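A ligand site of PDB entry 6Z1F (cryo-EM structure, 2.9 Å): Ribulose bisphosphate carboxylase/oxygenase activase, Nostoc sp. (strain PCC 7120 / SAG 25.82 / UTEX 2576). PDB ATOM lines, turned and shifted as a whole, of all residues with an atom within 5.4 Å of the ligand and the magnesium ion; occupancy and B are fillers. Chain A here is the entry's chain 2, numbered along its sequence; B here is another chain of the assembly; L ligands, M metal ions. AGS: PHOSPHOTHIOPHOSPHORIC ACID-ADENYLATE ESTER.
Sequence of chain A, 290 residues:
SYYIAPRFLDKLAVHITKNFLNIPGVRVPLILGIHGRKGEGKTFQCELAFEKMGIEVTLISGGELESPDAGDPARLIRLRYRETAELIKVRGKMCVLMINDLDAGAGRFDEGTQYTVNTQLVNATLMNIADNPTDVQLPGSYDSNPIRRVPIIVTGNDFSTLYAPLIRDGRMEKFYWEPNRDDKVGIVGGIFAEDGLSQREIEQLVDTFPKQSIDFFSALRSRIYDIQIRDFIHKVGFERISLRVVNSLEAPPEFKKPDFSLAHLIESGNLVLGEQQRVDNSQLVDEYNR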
ATOM      1  N   TYR A   2       4.047 -29.636  40.890  1.00  0.00           N
ATOM      2  CA  TYR A   2       4.925 -28.864  40.023  1.00  0.00           C
ATOM      3  C   TYR A   2       5.439 -27.635  40.770  1.00  0.00           C
ATOM      4  O   TYR A   2       4.681 -26.960  41.463  1.00  0.00           O
ATOM      5  CB  TYR A   2       4.192 -28.449  38.744  1.00  0.00           C
ATOM      6  CG  TYR A   2       3.896 -29.593  37.801  1.00  0.00           C
ATOM      7  CD1 TYR A   2       4.866 -30.088  36.951  1.00  0.00           C
ATOM      8  CD2 TYR A   2       2.631 -30.178  37.767  1.00  0.00           C
ATOM      9  CE1 TYR A   2       4.604 -31.132  36.084  1.00  0.00           C
ATOM     10  CE2 TYR A   2       2.356 -31.227  36.901  1.00  0.00           C
ATOM     11  CZ  TYR A   2       3.343 -31.708  36.052  1.00  0.00           C
ATOM     12  OH  TYR A   2       3.083 -32.735  35.202  1.00  0.00           O
ATOM     13  N   TYR A   3       6.733 -27.371  40.582  1.00  0.00           N
ATOM     14  CA  TYR A   3       7.434 -26.262  41.225  1.00  0.00           C
ATOM     15  C   TYR A   3       7.247 -24.999  40.392  1.00  0.00           C
ATOM     16  O   TYR A   3       7.393 -25.033  39.175  1.00  0.00           O
ATOM     17  CB  TYR A   3       8.897 -26.649  41.434  1.00  0.00           C
ATOM     18  CG  TYR A   3       9.792 -25.577  42.026  1.00  0.00           C
ATOM     19  CD1 TYR A   3       9.843 -25.358  43.390  1.00  0.00           C
ATOM     20  CD2 TYR A   3      10.627 -24.820  41.208  1.00  0.00           C
ATOM     21  CE1 TYR A   3      10.669 -24.389  43.937  1.00  0.00           C
ATOM     22  CE2 TYR A   3      11.457 -23.847  41.733  1.00  0.00           C
ATOM     23  CZ  TYR A   3      11.486 -23.630  43.102  1.00  0.00           C
ATOM     24  OH  TYR A   3      12.309 -22.674  43.622  1.00  0.00           O
ATOM     25  N   ARG A  37      13.319 -16.757  25.962  1.00  0.00           N
ATOM     26  CA  ARG A  37      13.637 -17.780  24.984  1.00  0.00           C
ATOM     27  C   ARG A  37      12.536 -18.837  24.954  1.00  0.00           C
ATOM     28  O   ARG A  37      11.807 -19.000  25.927  1.00  0.00           O
ATOM     29  CB  ARG A  37      14.983 -18.437  25.301  1.00  0.00           C
ATOM     30  CG  ARG A  37      16.193 -17.565  24.977  1.00  0.00           C
ATOM     31  CD  ARG A  37      17.496 -18.343  25.015  1.00  0.00           C
ATOM     32  NE  ARG A  37      17.788 -18.928  26.323  1.00  0.00           N
ATOM     33  CZ  ARG A  37      18.348 -18.280  27.347  1.00  0.00           C
ATOM     34  NH1 ARG A  37      18.559 -18.928  28.483  1.00  0.00           N
ATOM     35  NH2 ARG A  37      18.701 -17.014  27.244  1.00  0.00           N
ATOM     36  N   LYS A  38      12.439 -19.533  23.821  1.00  0.00           N
ATOM     37  CA  LYS A  38      11.416 -20.529  23.554  1.00  0.00           C
ATOM     38  C   LYS A  38      11.541 -21.708  24.523  1.00  0.00           C
ATOM     39  O   LYS A  38      12.636 -22.199  24.769  1.00  0.00           O
ATOM     40  CB  LYS A  38      11.464 -20.987  22.093  1.00  0.00           C
ATOM     41  CG  LYS A  38      12.832 -21.400  21.565  1.00  0.00           C
ATOM     42  CD  LYS A  38      12.822 -21.794  20.100  1.00  0.00           C
ATOM     43  CE  LYS A  38      14.154 -22.315  19.614  1.00  0.00           C
ATOM     44  NZ  LYS A  38      14.063 -22.866  18.239  1.00  0.00           N
ATOM     45  N   GLY A  39      10.391 -22.102  25.088  1.00  0.00           N
ATOM     46  CA  GLY A  39      10.267 -23.276  25.943  1.00  0.00           C
ATOM     47  C   GLY A  39      11.044 -23.156  27.246  1.00  0.00           C
ATOM     48  O   GLY A  39      11.641 -24.129  27.709  1.00  0.00           O
ATOM     49  N   GLU A  40      11.021 -21.957  27.847  1.00  0.00           N
ATOM     50  CA  GLU A  40      11.711 -21.675  29.092  1.00  0.00           C
ATOM     51  C   GLU A  40      10.714 -21.653  30.247  1.00  0.00           C
ATOM     52  O   GLU A  40      11.116 -21.620  31.408  1.00  0.00           O
ATOM     53  CB  GLU A  40      12.498 -20.366  28.978  1.00  0.00           C
ATOM     54  CG  GLU A  40      13.760 -20.487  28.128  1.00  0.00           C
ATOM     55  CD  GLU A  40      15.028 -20.954  28.848  1.00  0.00           C
ATOM     56  OE1 GLU A  40      15.005 -22.049  29.446  1.00  0.00           O
ATOM     57  OE2 GLU A  40      16.032 -20.217  28.796  1.00  0.00           O
ATOM     58  N   GLY A  41       9.423 -21.693  29.905  1.00  0.00           N
ATOM     59  CA  GLY A  41       8.347 -21.811  30.880  1.00  0.00           C
ATOM     60  C   GLY A  41       7.667 -20.474  31.155  1.00  0.00           C
ATOM     61  O   GLY A  41       7.628 -20.025  32.301  1.00  0.00           O
ATOM     62  N   LYS A  42       7.117 -19.865  30.096  1.00  0.00           N
ATOM     63  CA  LYS A  42       6.460 -18.581  30.190  1.00  0.00           C
ATOM     64  C   LYS A  42       4.945 -18.771  30.295  1.00  0.00           C
ATOM     65  O   LYS A  42       4.288 -18.148  31.120  1.00  0.00           O
ATOM     66  CB  LYS A  42       6.785 -17.706  28.980  1.00  0.00           C
ATOM     67  CG  LYS A  42       8.231 -17.256  28.851  1.00  0.00           C
ATOM     68  CD  LYS A  42       8.408 -16.152  27.823  1.00  0.00           C
ATOM     69  CE  LYS A  42       8.222 -16.632  26.399  1.00  0.00           C
ATOM     70  NZ  LYS A  42       9.467 -17.181  25.836  1.00  0.00           N
ATOM     71  N   THR A  43       4.406 -19.645  29.430  1.00  0.00           N
ATOM     72  CA  THR A  43       2.977 -19.890  29.371  1.00  0.00           C
ATOM     73  C   THR A  43       2.582 -20.882  30.464  1.00  0.00           C
ATOM     74  O   THR A  43       1.567 -20.690  31.117  1.00  0.00           O
ATOM     75  CB  THR A  43       2.564 -20.408  27.988  1.00  0.00           C
ATOM     76  OG1 THR A  43       3.275 -19.686  26.976  1.00  0.00           O
ATOM     77  CG2 THR A  43       1.075 -20.284  27.737  1.00  0.00           C
ATOM     78  N   PHE A  44       3.412 -21.920  30.624  1.00  0.00           N
ATOM     79  CA  PHE A  44       3.152 -23.032  31.537  1.00  0.00           C
ATOM     80  C   PHE A  44       3.093 -22.530  32.984  1.00  0.00           C
ATOM     81  O   PHE A  44       2.225 -22.955  33.743  1.00  0.00           O
ATOM     82  CB  PHE A  44       4.205 -24.120  31.358  1.00  0.00           C
ATOM     83  CG  PHE A  44       3.912 -25.414  32.075  1.00  0.00           C
ATOM     84  CD1 PHE A  44       3.200 -26.432  31.459  1.00  0.00           C
ATOM     85  CD2 PHE A  44       4.342 -25.607  33.382  1.00  0.00           C
ATOM     86  CE1 PHE A  44       2.924 -27.607  32.131  1.00  0.00           C
ATOM     87  CE2 PHE A  44       4.061 -26.791  34.052  1.00  0.00           C
ATOM     88  CZ  PHE A  44       3.351 -27.797  33.430  1.00  0.00           C
ATOM     89  N   GLN A  45       4.021 -21.638  33.343  1.00  0.00           N
ATOM     90  CA  GLN A  45       4.183 -21.203  34.722  1.00  0.00           C
ATOM     91  C   GLN A  45       3.068 -20.237  35.121  1.00  0.00           C
ATOM     92  O   GLN A  45       2.703 -20.185  36.288  1.00  0.00           O
ATOM     93  CB  GLN A  45       5.561 -20.576  34.944  1.00  0.00           C
ATOM     94  CG  GLN A  45       6.648 -21.601  35.223  1.00  0.00           C
ATOM     95  CD  GLN A  45       7.863 -20.984  35.855  1.00  0.00           C
ATOM     96  OE1 GLN A  45       7.802 -20.416  36.943  1.00  0.00           O
ATOM     97  NE2 GLN A  45       8.991 -21.085  35.167  1.00  0.00           N
ATOM     98  N   LEU A  48       0.083 -22.219  36.307  1.00  0.00           N
ATOM     99  CA  LEU A  48       0.298 -22.762  37.639  1.00  0.00           C
ATOM    100  C   LEU A  48       0.029 -21.694  38.700  1.00  0.00           C
ATOM    101  O   LEU A  48      -0.476 -22.007  39.779  1.00  0.00           O
ATOM    102  CB  LEU A  48       1.742 -23.252  37.756  1.00  0.00           C
ATOM    103  CG  LEU A  48       2.132 -24.492  36.939  1.00  0.00           C
ATOM    104  CD1 LEU A  48       3.641 -24.574  36.794  1.00  0.00           C
ATOM    105  CD2 LEU A  48       1.595 -25.763  37.593  1.00  0.00           C
ATOM    106  N   ASN A 100      -1.717 -14.506  24.592  1.00  0.00           N
ATOM    107  CA  ASN A 100      -0.527 -15.314  24.403  1.00  0.00           C
ATOM    108  C   ASN A 100      -0.057 -15.172  22.967  1.00  0.00           C
ATOM    109  O   ASN A 100      -0.875 -15.135  22.044  1.00  0.00           O
ATOM    110  CB  ASN A 100      -0.794 -16.772  24.795  1.00  0.00           C
ATOM    111  CG  ASN A 100       0.475 -17.600  24.909  1.00  0.00           C
ATOM    112  OD1 ASN A 100       1.417 -17.206  25.586  1.00  0.00           O
ATOM    113  ND2 ASN A 100       0.486 -18.745  24.255  1.00  0.00           N
ATOM    114  N   THR A 155       2.455 -12.416  26.721  1.00  0.00           N
ATOM    115  CA  THR A 155       3.600 -13.287  26.507  1.00  0.00           C
ATOM    116  C   THR A 155       4.019 -13.249  25.042  1.00  0.00           C
ATOM    117  O   THR A 155       3.184 -13.258  24.150  1.00  0.00           O
ATOM    118  CB  THR A 155       3.289 -14.714  26.988  1.00  0.00           C
ATOM    119  OG1 THR A 155       2.881 -14.626  28.356  1.00  0.00           O
ATOM    120  CG2 THR A 155       4.461 -15.649  26.874  1.00  0.00           C
ATOM    121  N   GLY A 156       5.346 -13.220  24.820  1.00  0.00           N
ATOM    122  CA  GLY A 156       5.917 -13.213  23.482  1.00  0.00           C
ATOM    123  C   GLY A 156       7.370 -13.694  23.468  1.00  0.00           C
ATOM    124  O   GLY A 156       7.948 -13.980  24.516  1.00  0.00           O
ATOM    125  N   ASN A 157       7.951 -13.738  22.263  1.00  0.00           N
ATOM    126  CA  ASN A 157       9.296 -14.253  22.064  1.00  0.00           C
ATOM    127  C   ASN A 157      10.287 -13.104  21.958  1.00  0.00           C
ATOM    128  O   ASN A 157      11.347 -13.155  22.584  1.00  0.00           O
ATOM    129  CB  ASN A 157       9.373 -15.184  20.850  1.00  0.00           C
ATOM    130  CG  ASN A 157      10.698 -15.911  20.748  1.00  0.00           C
ATOM    131  OD1 ASN A 157      11.214 -16.414  21.735  1.00  0.00           O
ATOM    132  ND2 ASN A 157      11.231 -15.989  19.540  1.00  0.00           N
ATOM    133  N   ILE A 187      12.850 -26.922  39.165  1.00  0.00           N
ATOM    134  CA  ILE A 187      11.859 -27.246  38.153  1.00  0.00           C
ATOM    135  C   ILE A 187      12.065 -28.683  37.667  1.00  0.00           C
ATOM    136  O   ILE A 187      11.122 -29.469  37.662  1.00  0.00           O
ATOM    137  CB  ILE A 187      11.867 -26.200  37.010  1.00  0.00           C
ATOM    138  CG1 ILE A 187      11.341 -24.844  37.486  1.00  0.00           C
ATOM    139  CG2 ILE A 187      11.100 -26.701  35.785  1.00  0.00           C
ATOM    140  CD1 ILE A 187      11.731 -23.669  36.611  1.00  0.00           C
ATOM    141  N   ILE A 191       9.814 -32.335  37.938  1.00  0.00           N
ATOM    142  CA  ILE A 191       9.426 -33.209  36.848  1.00  0.00           C
ATOM    143  C   ILE A 191       9.679 -34.661  37.249  1.00  0.00           C
ATOM    144  O   ILE A 191       8.814 -35.524  37.051  1.00  0.00           O
ATOM    145  CB  ILE A 191      10.121 -32.786  35.535  1.00  0.00           C
ATOM    146  CG1 ILE A 191       9.540 -31.478  34.991  1.00  0.00           C
ATOM    147  CG2 ILE A 191      10.069 -33.894  34.481  1.00  0.00           C
ATOM    148  CD1 ILE A 191      10.421 -30.755  34.005  1.00  0.00           C
ATOM    149  N   ILE A 214      13.854 -25.639  29.319  1.00  0.00           N
ATOM    150  CA  ILE A 214      13.162 -26.467  30.307  1.00  0.00           C
ATOM    151  C   ILE A 214      12.455 -27.626  29.612  1.00  0.00           C
ATOM    152  O   ILE A 214      12.407 -28.729  30.157  1.00  0.00           O
ATOM    153  CB  ILE A 214      12.206 -25.613  31.163  1.00  0.00           C
ATOM    154  CG1 ILE A 214      12.899 -24.395  31.796  1.00  0.00           C
ATOM    155  CG2 ILE A 214      11.459 -26.449  32.193  1.00  0.00           C
ATOM    156  CD1 ILE A 214      14.066 -24.705  32.713  1.00  0.00           C
ATOM    157  N   ASP A 215      11.944 -27.384  28.398  1.00  0.00           N
ATOM    158  CA  ASP A 215      11.188 -28.363  27.633  1.00  0.00           C
ATOM    159  C   ASP A 215      12.059 -29.565  27.277  1.00  0.00           C
ATOM    160  O   ASP A 215      11.538 -30.669  27.087  1.00  0.00           O
ATOM    161  CB  ASP A 215      10.531 -27.733  26.398  1.00  0.00           C
ATOM    162  CG  ASP A 215      11.493 -27.443  25.255  1.00  0.00           C
ATOM    163  OD1 ASP A 215      12.641 -27.029  25.537  1.00  0.00           O
ATOM    164  OD2 ASP A 215      11.086 -27.632  24.088  1.00  0.00           O
ATOM    165  N   SER A 218      11.738 -32.406  29.571  1.00  0.00           N
ATOM    166  CA  SER A 218      10.430 -33.031  29.465  1.00  0.00           C
ATOM    167  C   SER A 218      10.359 -33.941  28.230  1.00  0.00           C
ATOM    168  O   SER A 218       9.608 -34.914  28.226  1.00  0.00           O
ATOM    169  CB  SER A 218       9.321 -32.007  29.478  1.00  0.00           C
ATOM    170  OG  SER A 218       9.327 -31.224  28.298  1.00  0.00           O
ATOM    171  N   ARG B  27       3.691 -36.087  28.712  1.00  0.00           N
ATOM    172  CA  ARG B  27       3.408 -34.996  27.802  1.00  0.00           C
ATOM    173  C   ARG B  27       3.947 -35.350  26.417  1.00  0.00           C
ATOM    174  O   ARG B  27       5.150 -35.565  26.261  1.00  0.00           O
ATOM    175  CB  ARG B  27       4.022 -33.683  28.315  1.00  0.00           C
ATOM    176  CG  ARG B  27       3.404 -33.123  29.591  1.00  0.00           C
ATOM    177  CD  ARG B  27       1.970 -32.640  29.479  1.00  0.00           C
ATOM    178  NE  ARG B  27       1.777 -31.575  28.503  1.00  0.00           N
ATOM    179  CZ  ARG B  27       1.697 -30.281  28.781  1.00  0.00           C
ATOM    180  NH1 ARG B  27       1.796 -29.848  30.030  1.00  0.00           N
ATOM    181  NH2 ARG B  27       1.512 -29.404  27.806  1.00  0.00           N
ATOM    182  N   MET B 127       1.227 -23.283  16.041  1.00  0.00           N
ATOM    183  CA  MET B 127       1.710 -23.292  17.420  1.00  0.00           C
ATOM    184  C   MET B 127       0.547 -23.481  18.388  1.00  0.00           C
ATOM    185  O   MET B 127       0.719 -24.128  19.424  1.00  0.00           O
ATOM    186  CB  MET B 127       2.439 -21.983  17.738  1.00  0.00           C
ATOM    187  CG  MET B 127       3.867 -21.937  17.234  1.00  0.00           C
ATOM    188  SD  MET B 127       4.914 -20.777  18.155  1.00  0.00           S
ATOM    189  CE  MET B 127       4.283 -19.205  17.574  1.00  0.00           C
ATOM    190  N   ASP B 131      -0.462 -26.553  20.956  1.00  0.00           N
ATOM    191  CA  ASP B 131      -0.645 -26.242  22.359  1.00  0.00           C
ATOM    192  C   ASP B 131      -1.948 -26.854  22.863  1.00  0.00           C
ATOM    193  O   ASP B 131      -1.950 -27.547  23.879  1.00  0.00           O
ATOM    194  CB  ASP B 131      -0.578 -24.728  22.621  1.00  0.00           C
ATOM    195  CG  ASP B 131       0.828 -24.166  22.778  1.00  0.00           C
ATOM    196  OD1 ASP B 131       1.806 -24.904  22.502  1.00  0.00           O
ATOM    197  OD2 ASP B 131       0.940 -22.992  23.193  1.00  0.00           O
ATOM    198  N   PRO B 165      10.159 -20.826  17.469  1.00  0.00           N
ATOM    199  CA  PRO B 165       9.353 -21.394  18.553  1.00  0.00           C
ATOM    200  C   PRO B 165       8.430 -22.545  18.168  1.00  0.00           C
ATOM    201  O   PRO B 165       7.942 -23.257  19.041  1.00  0.00           O
ATOM    202  CB  PRO B 165       8.497 -20.207  19.021  1.00  0.00           C
ATOM    203  CG  PRO B 165       9.297 -19.000  18.631  1.00  0.00           C
ATOM    204  CD  PRO B 165       9.922 -19.380  17.315  1.00  0.00           C
ATOM    205  N   ARG B 168      10.434 -26.885  18.467  1.00  0.00           N
ATOM    206  CA  ARG B 168      11.066 -27.224  19.734  1.00  0.00           C
ATOM    207  C   ARG B 168      10.604 -28.610  20.169  1.00  0.00           C
ATOM    208  O   ARG B 168       9.542 -29.073  19.748  1.00  0.00           O
ATOM    209  CB  ARG B 168      10.865 -26.117  20.783  1.00  0.00           C
ATOM    210  CG  ARG B 168       9.422 -25.912  21.236  1.00  0.00           C
ATOM    211  CD  ARG B 168       9.274 -25.097  22.499  1.00  0.00           C
ATOM    212  NE  ARG B 168       8.136 -25.594  23.251  1.00  0.00           N
ATOM    213  CZ  ARG B 168       7.319 -24.858  23.994  1.00  0.00           C
ATOM    214  NH1 ARG B 168       6.310 -25.433  24.629  1.00  0.00           N
ATOM    215  NH2 ARG B 168       7.494 -23.549  24.094  1.00  0.00           N
ATOM    216  N   ARG B 171       7.049 -29.177  21.282  1.00  0.00           N
ATOM    217  CA  ARG B 171       5.986 -28.803  20.365  1.00  0.00           C
ATOM    218  C   ARG B 171       5.982 -29.690  19.133  1.00  0.00           C
ATOM    219  O   ARG B 171       4.933 -29.903  18.532  1.00  0.00           O
ATOM    220  CB  ARG B 171       6.139 -27.327  19.985  1.00  0.00           C
ATOM    221  CG  ARG B 171       4.826 -26.612  19.694  1.00  0.00           C
ATOM    222  CD  ARG B 171       5.105 -25.232  19.147  1.00  0.00           C
ATOM    223  NE  ARG B 171       5.521 -24.287  20.180  1.00  0.00           N
ATOM    224  CZ  ARG B 171       4.684 -23.529  20.881  1.00  0.00           C
ATOM    225  NH1 ARG B 171       3.375 -23.611  20.681  1.00  0.00           N
ATOM    226  NH2 ARG B 171       5.155 -22.706  21.798  1.00  0.00           N
HETATM  227  PG  AGS L   1       7.313 -20.009  23.697  1.00  0.00           P
HETATM  228  S1G AGS L   1       7.331 -20.914  22.453  1.00  0.00           S
HETATM  229  O2G AGS L   1       5.788 -19.598  23.888  1.00  0.00           O
HETATM  230  O3G AGS L   1       8.210 -18.815  23.598  1.00  0.00           O
HETATM  231  PB  AGS L   1       7.386 -20.757  26.404  1.00  0.00           P
HETATM  232  O1B AGS L   1       8.412 -19.964  27.108  1.00  0.00           O
HETATM  233  O2B AGS L   1       5.941 -20.059  26.490  1.00  0.00           O
HETATM  234  O3B AGS L   1       7.724 -21.021  24.884  1.00  0.00           O
HETATM  235  PA  AGS L   1       5.945 -22.839  27.694  1.00  0.00           P
HETATM  236  O1A AGS L   1       5.643 -22.238  29.008  1.00  0.00           O
HETATM  237  O2A AGS L   1       4.770 -22.622  26.588  1.00  0.00           O
HETATM  238  O3A AGS L   1       7.287 -22.240  27.043  1.00  0.00           O
HETATM  239  O5' AGS L   1       6.087 -24.439  27.788  1.00  0.00           O
HETATM  240  C5' AGS L   1       7.341 -25.086  28.065  1.00  0.00           C
HETATM  241  C4' AGS L   1       7.169 -26.611  28.154  1.00  0.00           C
HETATM  242  O4' AGS L   1       8.213 -27.099  29.020  1.00  0.00           O
HETATM  243  C3' AGS L   1       5.851 -26.980  28.846  1.00  0.00           C
HETATM  244  O3' AGS L   1       4.896 -27.423  27.867  1.00  0.00           O
HETATM  245  C2' AGS L   1       6.222 -28.106  29.810  1.00  0.00           C
HETATM  246  O2' AGS L   1       6.258 -29.388  29.151  1.00  0.00           O
HETATM  247  C1' AGS L   1       7.630 -27.740  30.219  1.00  0.00           C
HETATM  248  N9  AGS L   1       7.673 -26.890  31.471  1.00  0.00           N
HETATM  249  C8  AGS L   1       7.976 -25.603  31.510  1.00  0.00           C
HETATM  250  N7  AGS L   1       7.933 -25.196  32.773  1.00  0.00           N
HETATM  251  C5  AGS L   1       7.606 -26.246  33.540  1.00  0.00           C
HETATM  252  C6  AGS L   1       7.424 -26.363  34.871  1.00  0.00           C
HETATM  253  N6  AGS L   1       7.599 -25.278  35.621  1.00  0.00           N
HETATM  254  N1  AGS L   1       7.084 -27.535  35.438  1.00  0.00           N
HETATM  255  C2  AGS L   1       6.923 -28.650  34.607  1.00  0.00           C
HETATM  256  N3  AGS L   1       7.109 -28.497  33.222  1.00  0.00           N
HETATM  257  C4  AGS L   1       7.450 -27.298  32.720  1.00  0.00           C
HETATM  258 MG    MG M   1       4.302 -20.076  24.897  1.00  0.00          MG
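N of Gly 39 is in hydrogen-bond range of O3B of the ligand, at 2.9 Å. An oxygen (O2A) of the ligand lies within salt-bridge range of the guanidinium group (NH1) of Arg 168 of chain B (3.8 Å). An oxygen (O1A) of the ligand is in hydrogen-bond range of the backbone NH of Phe 44, at 2.8 Å. A sulfur (S1G) of the ligand sits close to the guanidinium group (NH2) of Arg 171 of chain B (2.9 Å). The backbone NH (N) of Gly 41 lies within hydrogen-bond range of an oxygen (O1B) of the ligand (3.4 Å). An oxygen (O1B) of the ligand is in hydrogen-bond range of the backbone NH (N) of Glu 40, at 3.4 Å. The side-chain amino group (NZ) of Lys 42 is in salt-bridge range of an oxygen (O1B) of the ligand, at 3.2 Å. N of Lys 42 is in hydrogen-bond range of O1A of the ligand (3.0 Å). The backbone NH (N) of Thr 43 sits at hydrogen-bond distance from an oxygen (O1A) of the ligand (2.9 Å).
The backbone carbonyl oxygen of Arg 37 is in hydrogen-bond range of the side-chain amino group of Lys 42 (3.0 Å). The backbone carbonyl oxygen (O) of Gly 39 sits at hydrogen-bond distance from the backbone NH (N) of Asp 215 (3.3 Å). The guanidinium group (NH1) of Arg 171 of chain B is in hydrogen-bond range of the backbone carbonyl oxygen (O) of Met 127 of chain B, 3.0 Å away. The side-chain carboxylate (OD2) of Asp 215 is in salt-bridge range of the guanidinium group (NE) of Arg 168 of chain B (3.7 Å). The side-chain carboxylate (OE2) of Glu 40 is in salt-bridge range of the guanidinium group (NH1) of Arg 37 (2.9 Å). The side-chain hydroxyl (OG) of Ser 218 is in hydrogen-bond range of the backbone carbonyl oxygen (O) of Asp 215, at 2.6 Å. The backbone carbonyl oxygen of Gly 39 is in hydrogen-bond range of the backbone NH of Ile 214 (3.1 Å). The side-chain carboxylate of Asp 131 of chain B is in salt-bridge range of the guanidinium group of Arg 171 of chain B, 2.7 Å away.
Tyr 2 touches the ligand (CD1 to C2, 3.4 Å). Tyr 3 touches the ligand (O to N6, 3.6 Å). Arg 37 touches the ligand (O to O1B, 3.7 Å). Lys 38 touches the ligand (CA to O3G, 3.6 Å). CG of Gln 45 touches N6 of the ligand, at 3.8 Å. Ile 187 touches the ligand (CG2 to N6, 3.8 Å). CG1 of Ile 191 touches C2 of the ligand, at 3.9 Å. CG2 of Ile 214 touches C8 of the ligand (3.6 Å). Asp 215 touches the ligand (CA to O4', 3.5 Å). Ser 218 touches the ligand (OG to O2', 3.7 Å). NH2 of Arg 27 of chain B touches O3' of the ligand, at 3.9 Å. Pro 165 of chain B touches the ligand. Hydrophobic or aromatic side chains within 4 Å of the ligand: Tyr 2, Phe 44, Ile 187, Ile 191, Ile 214 and Pro 165 of chain B. The nearest printed residue that does not touch the ligand is Leu 48 (4.2 Å).
The nearest printed residue that does not touch the magnesium ion is Asn 100 (4.1 Å).
An oxygen (O2G) of the ligand binds the magnesium ion (1.9 Å). The magnesium ion is bound by O2B of the ligand, at 2.3 Å. OG1 of Thr 43 is bound to the magnesium ion, 2.4 Å away. The magnesium ion has three donor atoms within binding distance.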
